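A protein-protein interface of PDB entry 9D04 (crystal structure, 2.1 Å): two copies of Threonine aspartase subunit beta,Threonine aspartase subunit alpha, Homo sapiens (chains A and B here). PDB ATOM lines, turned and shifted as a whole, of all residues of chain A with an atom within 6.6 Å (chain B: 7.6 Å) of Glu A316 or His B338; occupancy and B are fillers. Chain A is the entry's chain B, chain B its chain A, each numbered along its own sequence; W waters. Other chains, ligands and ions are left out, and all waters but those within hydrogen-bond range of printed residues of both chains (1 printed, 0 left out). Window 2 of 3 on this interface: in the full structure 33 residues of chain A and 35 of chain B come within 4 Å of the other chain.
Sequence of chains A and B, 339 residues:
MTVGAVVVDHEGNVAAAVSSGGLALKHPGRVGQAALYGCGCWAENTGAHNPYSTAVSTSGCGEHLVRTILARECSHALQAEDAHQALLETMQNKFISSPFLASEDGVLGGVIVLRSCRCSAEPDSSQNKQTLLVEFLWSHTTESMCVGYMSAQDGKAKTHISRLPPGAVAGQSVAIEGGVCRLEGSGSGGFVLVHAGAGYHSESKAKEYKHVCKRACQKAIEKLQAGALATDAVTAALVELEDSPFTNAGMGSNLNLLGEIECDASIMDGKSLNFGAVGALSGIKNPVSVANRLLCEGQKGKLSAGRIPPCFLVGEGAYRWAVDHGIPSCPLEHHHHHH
Water W1 bridges N of Glu A316 (3.4 Å) and N of Glu B316 (3.5 Å).
Val A314 touches its own counterpart, Val B314.
Of the 8 pairs that touch across the chains among the printed residues, 1 has its exchanged pair printed and touching as well.
The backbone carbonyl oxygen of Gly B29 lies within hydrogen-bond range of the backbone NH of Val A314 (2.9 Å).
The side-chain carboxylate of Glu A316 sits close to the backbone carbonyl oxygen of His B338 (3.4 Å).
The side-chain carboxylate of Glu A316 sits close to the backbone carbonyl oxygen of His B337, at 3.5 Å.
Printed residues of chain B that touch a printed residue of chain A: His B27, Pro B28, Gly B29, Val B314, His B337 and His B338.
Hydrophobic or aromatic side chains of chain B within 4 Å of the printed part of chain A: His B27, Val B314 and His B337.
Of the 12 printed residues of chain A, 5 touch a printed residue of chain B.
Printed residues of chain A that touch a printed residue of chain B: Ala A280, Val A314, Glu A316, Gly A317 and Trp A321.
Along chain A the printed residues that touch a printed residue of chain B span positions 280 to 321.
Among the printed residues, no Asp or Glu carboxylate lies within 4 Å of a Lys or Arg side-chain nitrogen of the other chain.
Of the printed residues of chain B, Glu A316 touches His B337 (3.2 Å) and His B338 (3.4 Å).
Gly A317 touches just these residues of chain B: His B27 and Pro B28.
Printed residues of chain B within 4 Å of Val A314: Gly B29 (2.9 Å) and Val B314 (3.9 Å).
Printed residues of chain B within 4 Å of Ala A280: Val B314.
Of the printed residues of chain A, His B337 touches Glu A316.
Printed residues of chain A within 4 Å of Val B314: Ala A280 and Val A314.
His B336 touches none of the printed residues of chain A.
The nearest printed residue of chain A that does not touch Gly B29 is Gly A317 (4.2 Å).
Among the printed residues, pairs that only touch across the chains: Ala A280 with Val B314, Val A314 with Val B314, Gly A317 with His B27, Gly A317 with Pro B28 and Trp A321 with His B27.
The backbone NH (N) of Gly B29 lies within hydrogen-bond range of the side-chain carboxylate (OE1) of Glu B262, 2.8 Å away.
The backbone carbonyl oxygen of Ala A280 sits close to the backbone NH of Gly A315 (3.4 Å).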
ATOM      1  N   GLY A 279      14.092  -6.570  25.870  1.00  0.00           N
ATOM      2  CA  GLY A 279      13.999  -5.217  26.380  1.00  0.00           C
ATOM      3  C   GLY A 279      13.352  -4.317  25.348  1.00  0.00           C
ATOM      4  O   GLY A 279      13.498  -4.515  24.141  1.00  0.00           O
ATOM      5  N   ALA A 280      12.626  -3.322  25.845  1.00  0.00           N
ATOM      6  CA  ALA A 280      11.968  -2.330  25.008  1.00  0.00           C
ATOM      7  C   ALA A 280      11.161  -3.001  23.895  1.00  0.00           C
ATOM      8  O   ALA A 280      11.234  -2.624  22.724  1.00  0.00           O
ATOM      9  CB  ALA A 280      12.987  -1.324  24.441  1.00  0.00           C
ATOM     10  N   LEU A 281      10.406  -4.036  24.269  1.00  0.00           N
ATOM     11  CA  LEU A 281       9.605  -4.799  23.313  1.00  0.00           C
ATOM     12  C   LEU A 281       8.193  -4.213  23.224  1.00  0.00           C
ATOM     13  O   LEU A 281       7.491  -4.116  24.239  1.00  0.00           O
ATOM     14  CB  LEU A 281       9.558  -6.273  23.727  1.00  0.00           C
ATOM     15  CG  LEU A 281       8.724  -7.197  22.826  1.00  0.00           C
ATOM     16  CD1 LEU A 281       9.312  -7.293  21.418  1.00  0.00           C
ATOM     17  CD2 LEU A 281       8.589  -8.572  23.468  1.00  0.00           C
ATOM     18  N   SER A 282       7.781  -3.806  22.028  1.00  0.00           N
ATOM     19  CA  SER A 282       6.428  -3.333  21.771  1.00  0.00           C
ATOM     20  C   SER A 282       5.715  -4.291  20.826  1.00  0.00           C
ATOM     21  O   SER A 282       6.345  -4.996  20.034  1.00  0.00           O
ATOM     22  CB  SER A 282       6.421  -1.924  21.148  1.00  0.00           C
ATOM     23  OG  SER A 282       7.092  -0.971  21.954  1.00  0.00           O
ATOM     24  N   VAL A 314      16.275  -6.778  21.756  1.00  0.00           N
ATOM     25  CA  VAL A 314      15.573  -5.552  22.105  1.00  0.00           C
ATOM     26  C   VAL A 314      14.850  -4.972  20.893  1.00  0.00           C
ATOM     27  O   VAL A 314      15.185  -5.244  19.734  1.00  0.00           O
ATOM     28  CB  VAL A 314      16.525  -4.499  22.705  1.00  0.00           C
ATOM     29  CG1 VAL A 314      17.219  -5.072  23.958  1.00  0.00           C
ATOM     30  CG2 VAL A 314      17.544  -4.000  21.637  1.00  0.00           C
ATOM     31  N   GLY A 315      13.836  -4.160  21.190  1.00  0.00           N
ATOM     32  CA  GLY A 315      13.227  -3.260  20.211  1.00  0.00           C
ATOM     33  C   GLY A 315      12.601  -3.988  19.044  1.00  0.00           C
ATOM     34  O   GLY A 315      12.021  -5.068  19.185  1.00  0.00           O
ATOM     35  N   GLU A 316      12.723  -3.371  17.867  1.00  0.00           N
ATOM     36  CA  GLU A 316      12.125  -3.898  16.643  1.00  0.00           C
ATOM     37  C   GLU A 316      12.700  -5.272  16.294  1.00  0.00           C
ATOM     38  O   GLU A 316      11.974  -6.162  15.831  1.00  0.00           O
ATOM     39  CB  GLU A 316      12.346  -2.900  15.504  1.00  0.00           C
ATOM     40  CG  GLU A 316      11.736  -3.265  14.152  1.00  0.00           C
ATOM     41  CD  GLU A 316      10.208  -3.271  14.173  1.00  0.00           C
ATOM     42  OE1 GLU A 316       9.617  -2.700  15.129  1.00  0.00           O
ATOM     43  OE2 GLU A 316       9.604  -3.815  13.210  1.00  0.00           O
ATOM     44  N   GLY A 317      14.003  -5.472  16.505  1.00  0.00           N
ATOM     45  CA  GLY A 317      14.559  -6.791  16.261  1.00  0.00           C
ATOM     46  C   GLY A 317      13.893  -7.864  17.114  1.00  0.00           C
ATOM     47  O   GLY A 317      13.571  -8.949  16.621  1.00  0.00           O
ATOM     48  N   ALA A 318      13.627  -7.556  18.389  1.00  0.00           N
ATOM     49  CA  ALA A 318      12.923  -8.506  19.246  1.00  0.00           C
ATOM     50  C   ALA A 318      11.502  -8.765  18.751  1.00  0.00           C
ATOM     51  O   ALA A 318      11.029  -9.906  18.774  1.00  0.00           O
ATOM     52  CB  ALA A 318      12.914  -8.011  20.688  1.00  0.00           C
ATOM     53  N   TYR A 319      10.800  -7.719  18.313  1.00  0.00           N
ATOM     54  CA  TYR A 319       9.455  -7.906  17.774  1.00  0.00           C
ATOM     55  C   TYR A 319       9.479  -8.822  16.552  1.00  0.00           C
ATOM     56  O   TYR A 319       8.706  -9.788  16.467  1.00  0.00           O
ATOM     57  CB  TYR A 319       8.842  -6.547  17.424  1.00  0.00           C
ATOM     58  CG  TYR A 319       7.523  -6.642  16.686  1.00  0.00           C
ATOM     59  CD1 TYR A 319       6.328  -6.806  17.371  1.00  0.00           C
ATOM     60  CD2 TYR A 319       7.480  -6.581  15.290  1.00  0.00           C
ATOM     61  CE1 TYR A 319       5.109  -6.892  16.687  1.00  0.00           C
ATOM     62  CE2 TYR A 319       6.272  -6.675  14.595  1.00  0.00           C
ATOM     63  CZ  TYR A 319       5.092  -6.828  15.299  1.00  0.00           C
ATOM     64  OH  TYR A 319       3.899  -6.918  14.612  1.00  0.00           O
ATOM     65  N   ARG A 320      10.363  -8.525  15.589  1.00  0.00           N
ATOM     66  CA  ARG A 320      10.456  -9.325  14.372  1.00  0.00           C
ATOM     67  C   ARG A 320      10.768 -10.787  14.687  1.00  0.00           C
ATOM     68  O   ARG A 320      10.176 -11.700  14.092  1.00  0.00           O
ATOM     69  CB  ARG A 320      11.525  -8.727  13.455  1.00  0.00           C
ATOM     70  CG  ARG A 320      11.660  -9.383  12.090  1.00  0.00           C
ATOM     71  CD  ARG A 320      10.312  -9.604  11.416  1.00  0.00           C
ATOM     72  NE  ARG A 320       9.492  -8.398  11.355  1.00  0.00           N
ATOM     73  CZ  ARG A 320       8.212  -8.399  11.004  1.00  0.00           C
ATOM     74  NH1 ARG A 320       7.619  -9.545  10.692  1.00  0.00           N
ATOM     75  NH2 ARG A 320       7.525  -7.263  10.964  1.00  0.00           N
ATOM     76  N   TRP A 321      11.691 -11.022  15.629  1.00  0.00           N
ATOM     77  CA  TRP A 321      12.032 -12.378  16.046  1.00  0.00           C
ATOM     78  C   TRP A 321      10.844 -13.080  16.698  1.00  0.00           C
ATOM     79  O   TRP A 321      10.584 -14.259  16.425  1.00  0.00           O
ATOM     80  CB  TRP A 321      13.220 -12.331  17.006  1.00  0.00           C
ATOM     81  CG  TRP A 321      13.845 -13.661  17.313  1.00  0.00           C
ATOM     82  CD1 TRP A 321      14.928 -14.211  16.699  1.00  0.00           C
ATOM     83  CD2 TRP A 321      13.453 -14.589  18.343  1.00  0.00           C
ATOM     84  NE1 TRP A 321      15.230 -15.430  17.273  1.00  0.00           N
ATOM     85  CE2 TRP A 321      14.332 -15.687  18.274  1.00  0.00           C
ATOM     86  CE3 TRP A 321      12.434 -14.605  19.300  1.00  0.00           C
ATOM     87  CZ2 TRP A 321      14.219 -16.794  19.123  1.00  0.00           C
ATOM     88  CZ3 TRP A 321      12.330 -15.702  20.145  1.00  0.00           C
ATOM     89  CH2 TRP A 321      13.220 -16.774  20.053  1.00  0.00           C
ATOM     90  N   HIS B  27      21.332 -11.544  14.715  1.00  0.00           N
ATOM     91  CA  HIS B  27      19.964 -11.120  14.498  1.00  0.00           C
ATOM     92  C   HIS B  27      19.802  -9.662  14.922  1.00  0.00           C
ATOM     93  O   HIS B  27      20.409  -9.231  15.909  1.00  0.00           O
ATOM     94  CB  HIS B  27      18.981 -11.997  15.278  1.00  0.00           C
ATOM     95  CG  HIS B  27      17.546 -11.761  14.908  1.00  0.00           C
ATOM     96  ND1 HIS B  27      16.818 -10.690  15.385  1.00  0.00           N
ATOM     97  CD2 HIS B  27      16.714 -12.438  14.082  1.00  0.00           C
ATOM     98  CE1 HIS B  27      15.591 -10.734  14.892  1.00  0.00           C
ATOM     99  NE2 HIS B  27      15.504 -11.783  14.094  1.00  0.00           N
ATOM    100  N   PRO B  28      19.007  -8.875  14.198  1.00  0.00           N
ATOM    101  CA  PRO B  28      18.745  -7.496  14.625  1.00  0.00           C
ATOM    102  C   PRO B  28      18.260  -7.459  16.064  1.00  0.00           C
ATOM    103  O   PRO B  28      17.448  -8.290  16.491  1.00  0.00           O
ATOM    104  CB  PRO B  28      17.657  -7.021  13.649  1.00  0.00           C
ATOM    105  CG  PRO B  28      17.885  -7.840  12.427  1.00  0.00           C
ATOM    106  CD  PRO B  28      18.334  -9.195  12.928  1.00  0.00           C
ATOM    107  N   GLY B  29      18.759  -6.480  16.811  1.00  0.00           N
ATOM    108  CA  GLY B  29      18.365  -6.273  18.184  1.00  0.00           C
ATOM    109  C   GLY B  29      19.097  -7.113  19.215  1.00  0.00           C
ATOM    110  O   GLY B  29      18.856  -6.923  20.413  1.00  0.00           O
ATOM    111  N   GLU B 262      24.692  -2.310  14.420  1.00  0.00           N
ATOM    112  CA  GLU B 262      24.055  -2.131  15.729  1.00  0.00           C
ATOM    113  C   GLU B 262      25.114  -2.245  16.810  1.00  0.00           C
ATOM    114  O   GLU B 262      25.712  -3.311  16.979  1.00  0.00           O
ATOM    115  CB  GLU B 262      22.936  -3.147  15.972  1.00  0.00           C
ATOM    116  CG  GLU B 262      21.633  -2.858  15.221  1.00  0.00           C
ATOM    117  CD  GLU B 262      20.551  -3.880  15.561  1.00  0.00           C
ATOM    118  OE1 GLU B 262      20.863  -5.089  15.594  1.00  0.00           O
ATOM    119  OE2 GLU B 262      19.403  -3.479  15.836  1.00  0.00           O
ATOM    120  N   VAL B 314      18.315   1.740  24.338  1.00  0.00           N
ATOM    121  CA  VAL B 314      18.564   0.869  23.193  1.00  0.00           C
ATOM    122  C   VAL B 314      17.814   1.374  21.963  1.00  0.00           C
ATOM    123  O   VAL B 314      16.839   2.117  22.060  1.00  0.00           O
ATOM    124  CB  VAL B 314      18.154  -0.595  23.451  1.00  0.00           C
ATOM    125  CG1 VAL B 314      18.932  -1.186  24.650  1.00  0.00           C
ATOM    126  CG2 VAL B 314      16.626  -0.685  23.612  1.00  0.00           C
ATOM    127  N   GLY B 315      18.298   0.951  20.795  1.00  0.00           N
ATOM    128  CA  GLY B 315      17.506   1.031  19.576  1.00  0.00           C
ATOM    129  C   GLY B 315      17.149   2.452  19.175  1.00  0.00           C
ATOM    130  O   GLY B 315      17.954   3.383  19.289  1.00  0.00           O
ATOM    131  N   GLU B 316      15.908   2.617  18.706  1.00  0.00           N
ATOM    132  CA  GLU B 316      15.454   3.908  18.185  1.00  0.00           C
ATOM    133  C   GLU B 316      15.496   5.000  19.245  1.00  0.00           C
ATOM    134  O   GLU B 316      15.955   6.120  18.976  1.00  0.00           O
ATOM    135  CB  GLU B 316      14.029   3.764  17.633  1.00  0.00           C
ATOM    136  CG  GLU B 316      13.375   5.084  17.175  1.00  0.00           C
ATOM    137  CD  GLU B 316      14.077   5.720  16.001  1.00  0.00           C
ATOM    138  OE1 GLU B 316      14.835   5.019  15.306  1.00  0.00           O
ATOM    139  OE2 GLU B 316      13.879   6.934  15.780  1.00  0.00           O
ATOM    140  N   HIS B 335      18.782   3.102  11.078  1.00  0.00           N
ATOM    141  CA  HIS B 335      17.624   2.371  10.585  1.00  0.00           C
ATOM    142  C   HIS B 335      16.544   2.339  11.661  1.00  0.00           C
ATOM    143  O   HIS B 335      16.834   2.381  12.865  1.00  0.00           O
ATOM    144  CB  HIS B 335      17.996   0.935  10.144  1.00  0.00           C
ATOM    145  CG  HIS B 335      18.824   0.183  11.146  1.00  0.00           C
ATOM    146  ND1 HIS B 335      18.287  -0.379  12.287  1.00  0.00           N
ATOM    147  CD2 HIS B 335      20.149  -0.102  11.176  1.00  0.00           C
ATOM    148  CE1 HIS B 335      19.244  -0.973  12.979  1.00  0.00           C
ATOM    149  NE2 HIS B 335      20.383  -0.823  12.326  1.00  0.00           N
ATOM    150  N   HIS B 336      15.292   2.277  11.207  1.00  0.00           N
ATOM    151  CA  HIS B 336      14.117   2.260  12.079  1.00  0.00           C
ATOM    152  C   HIS B 336      13.012   1.542  11.302  1.00  0.00           C
ATOM    153  O   HIS B 336      12.241   2.170  10.576  1.00  0.00           O
ATOM    154  CB  HIS B 336      13.699   3.668  12.484  1.00  0.00           C
ATOM    155  CG  HIS B 336      12.468   3.718  13.343  1.00  0.00           C
ATOM    156  ND1 HIS B 336      12.212   2.795  14.337  1.00  0.00           N
ATOM    157  CD2 HIS B 336      11.437   4.595  13.369  1.00  0.00           C
ATOM    158  CE1 HIS B 336      11.067   3.094  14.927  1.00  0.00           C
ATOM    159  NE2 HIS B 336      10.578   4.182  14.359  1.00  0.00           N
ATOM    160  N   HIS B 337      12.952   0.224  11.463  1.00  0.00           N
ATOM    161  CA  HIS B 337      12.028  -0.598  10.696  1.00  0.00           C
ATOM    162  C   HIS B 337      10.667  -0.689  11.383  1.00  0.00           C
ATOM    163  O   HIS B 337      10.540  -0.527  12.599  1.00  0.00           O
ATOM    164  CB  HIS B 337      12.607  -1.998  10.484  1.00  0.00           C
ATOM    165  CG  HIS B 337      13.903  -2.011   9.733  1.00  0.00           C
ATOM    166  ND1 HIS B 337      14.008  -1.598   8.421  1.00  0.00           N
ATOM    167  CD2 HIS B 337      15.149  -2.390  10.108  1.00  0.00           C
ATOM    168  CE1 HIS B 337      15.261  -1.722   8.021  1.00  0.00           C
ATOM    169  NE2 HIS B 337      15.973  -2.200   9.025  1.00  0.00           N
ATOM    170  N   HIS B 338       9.642  -0.952  10.578  1.00  0.00           N
ATOM    171  CA  HIS B 338       8.280  -1.102  11.078  1.00  0.00           C
ATOM    172  C   HIS B 338       7.602  -2.304  10.433  1.00  0.00           C
ATOM    173  O   HIS B 338       7.030  -3.149  11.119  1.00  0.00           O
ATOM    174  CB  HIS B 338       7.465   0.169  10.818  1.00  0.00           C
HETATM  175  O   HOH W   1      14.468  -0.528  18.183  1.00  0.00           O
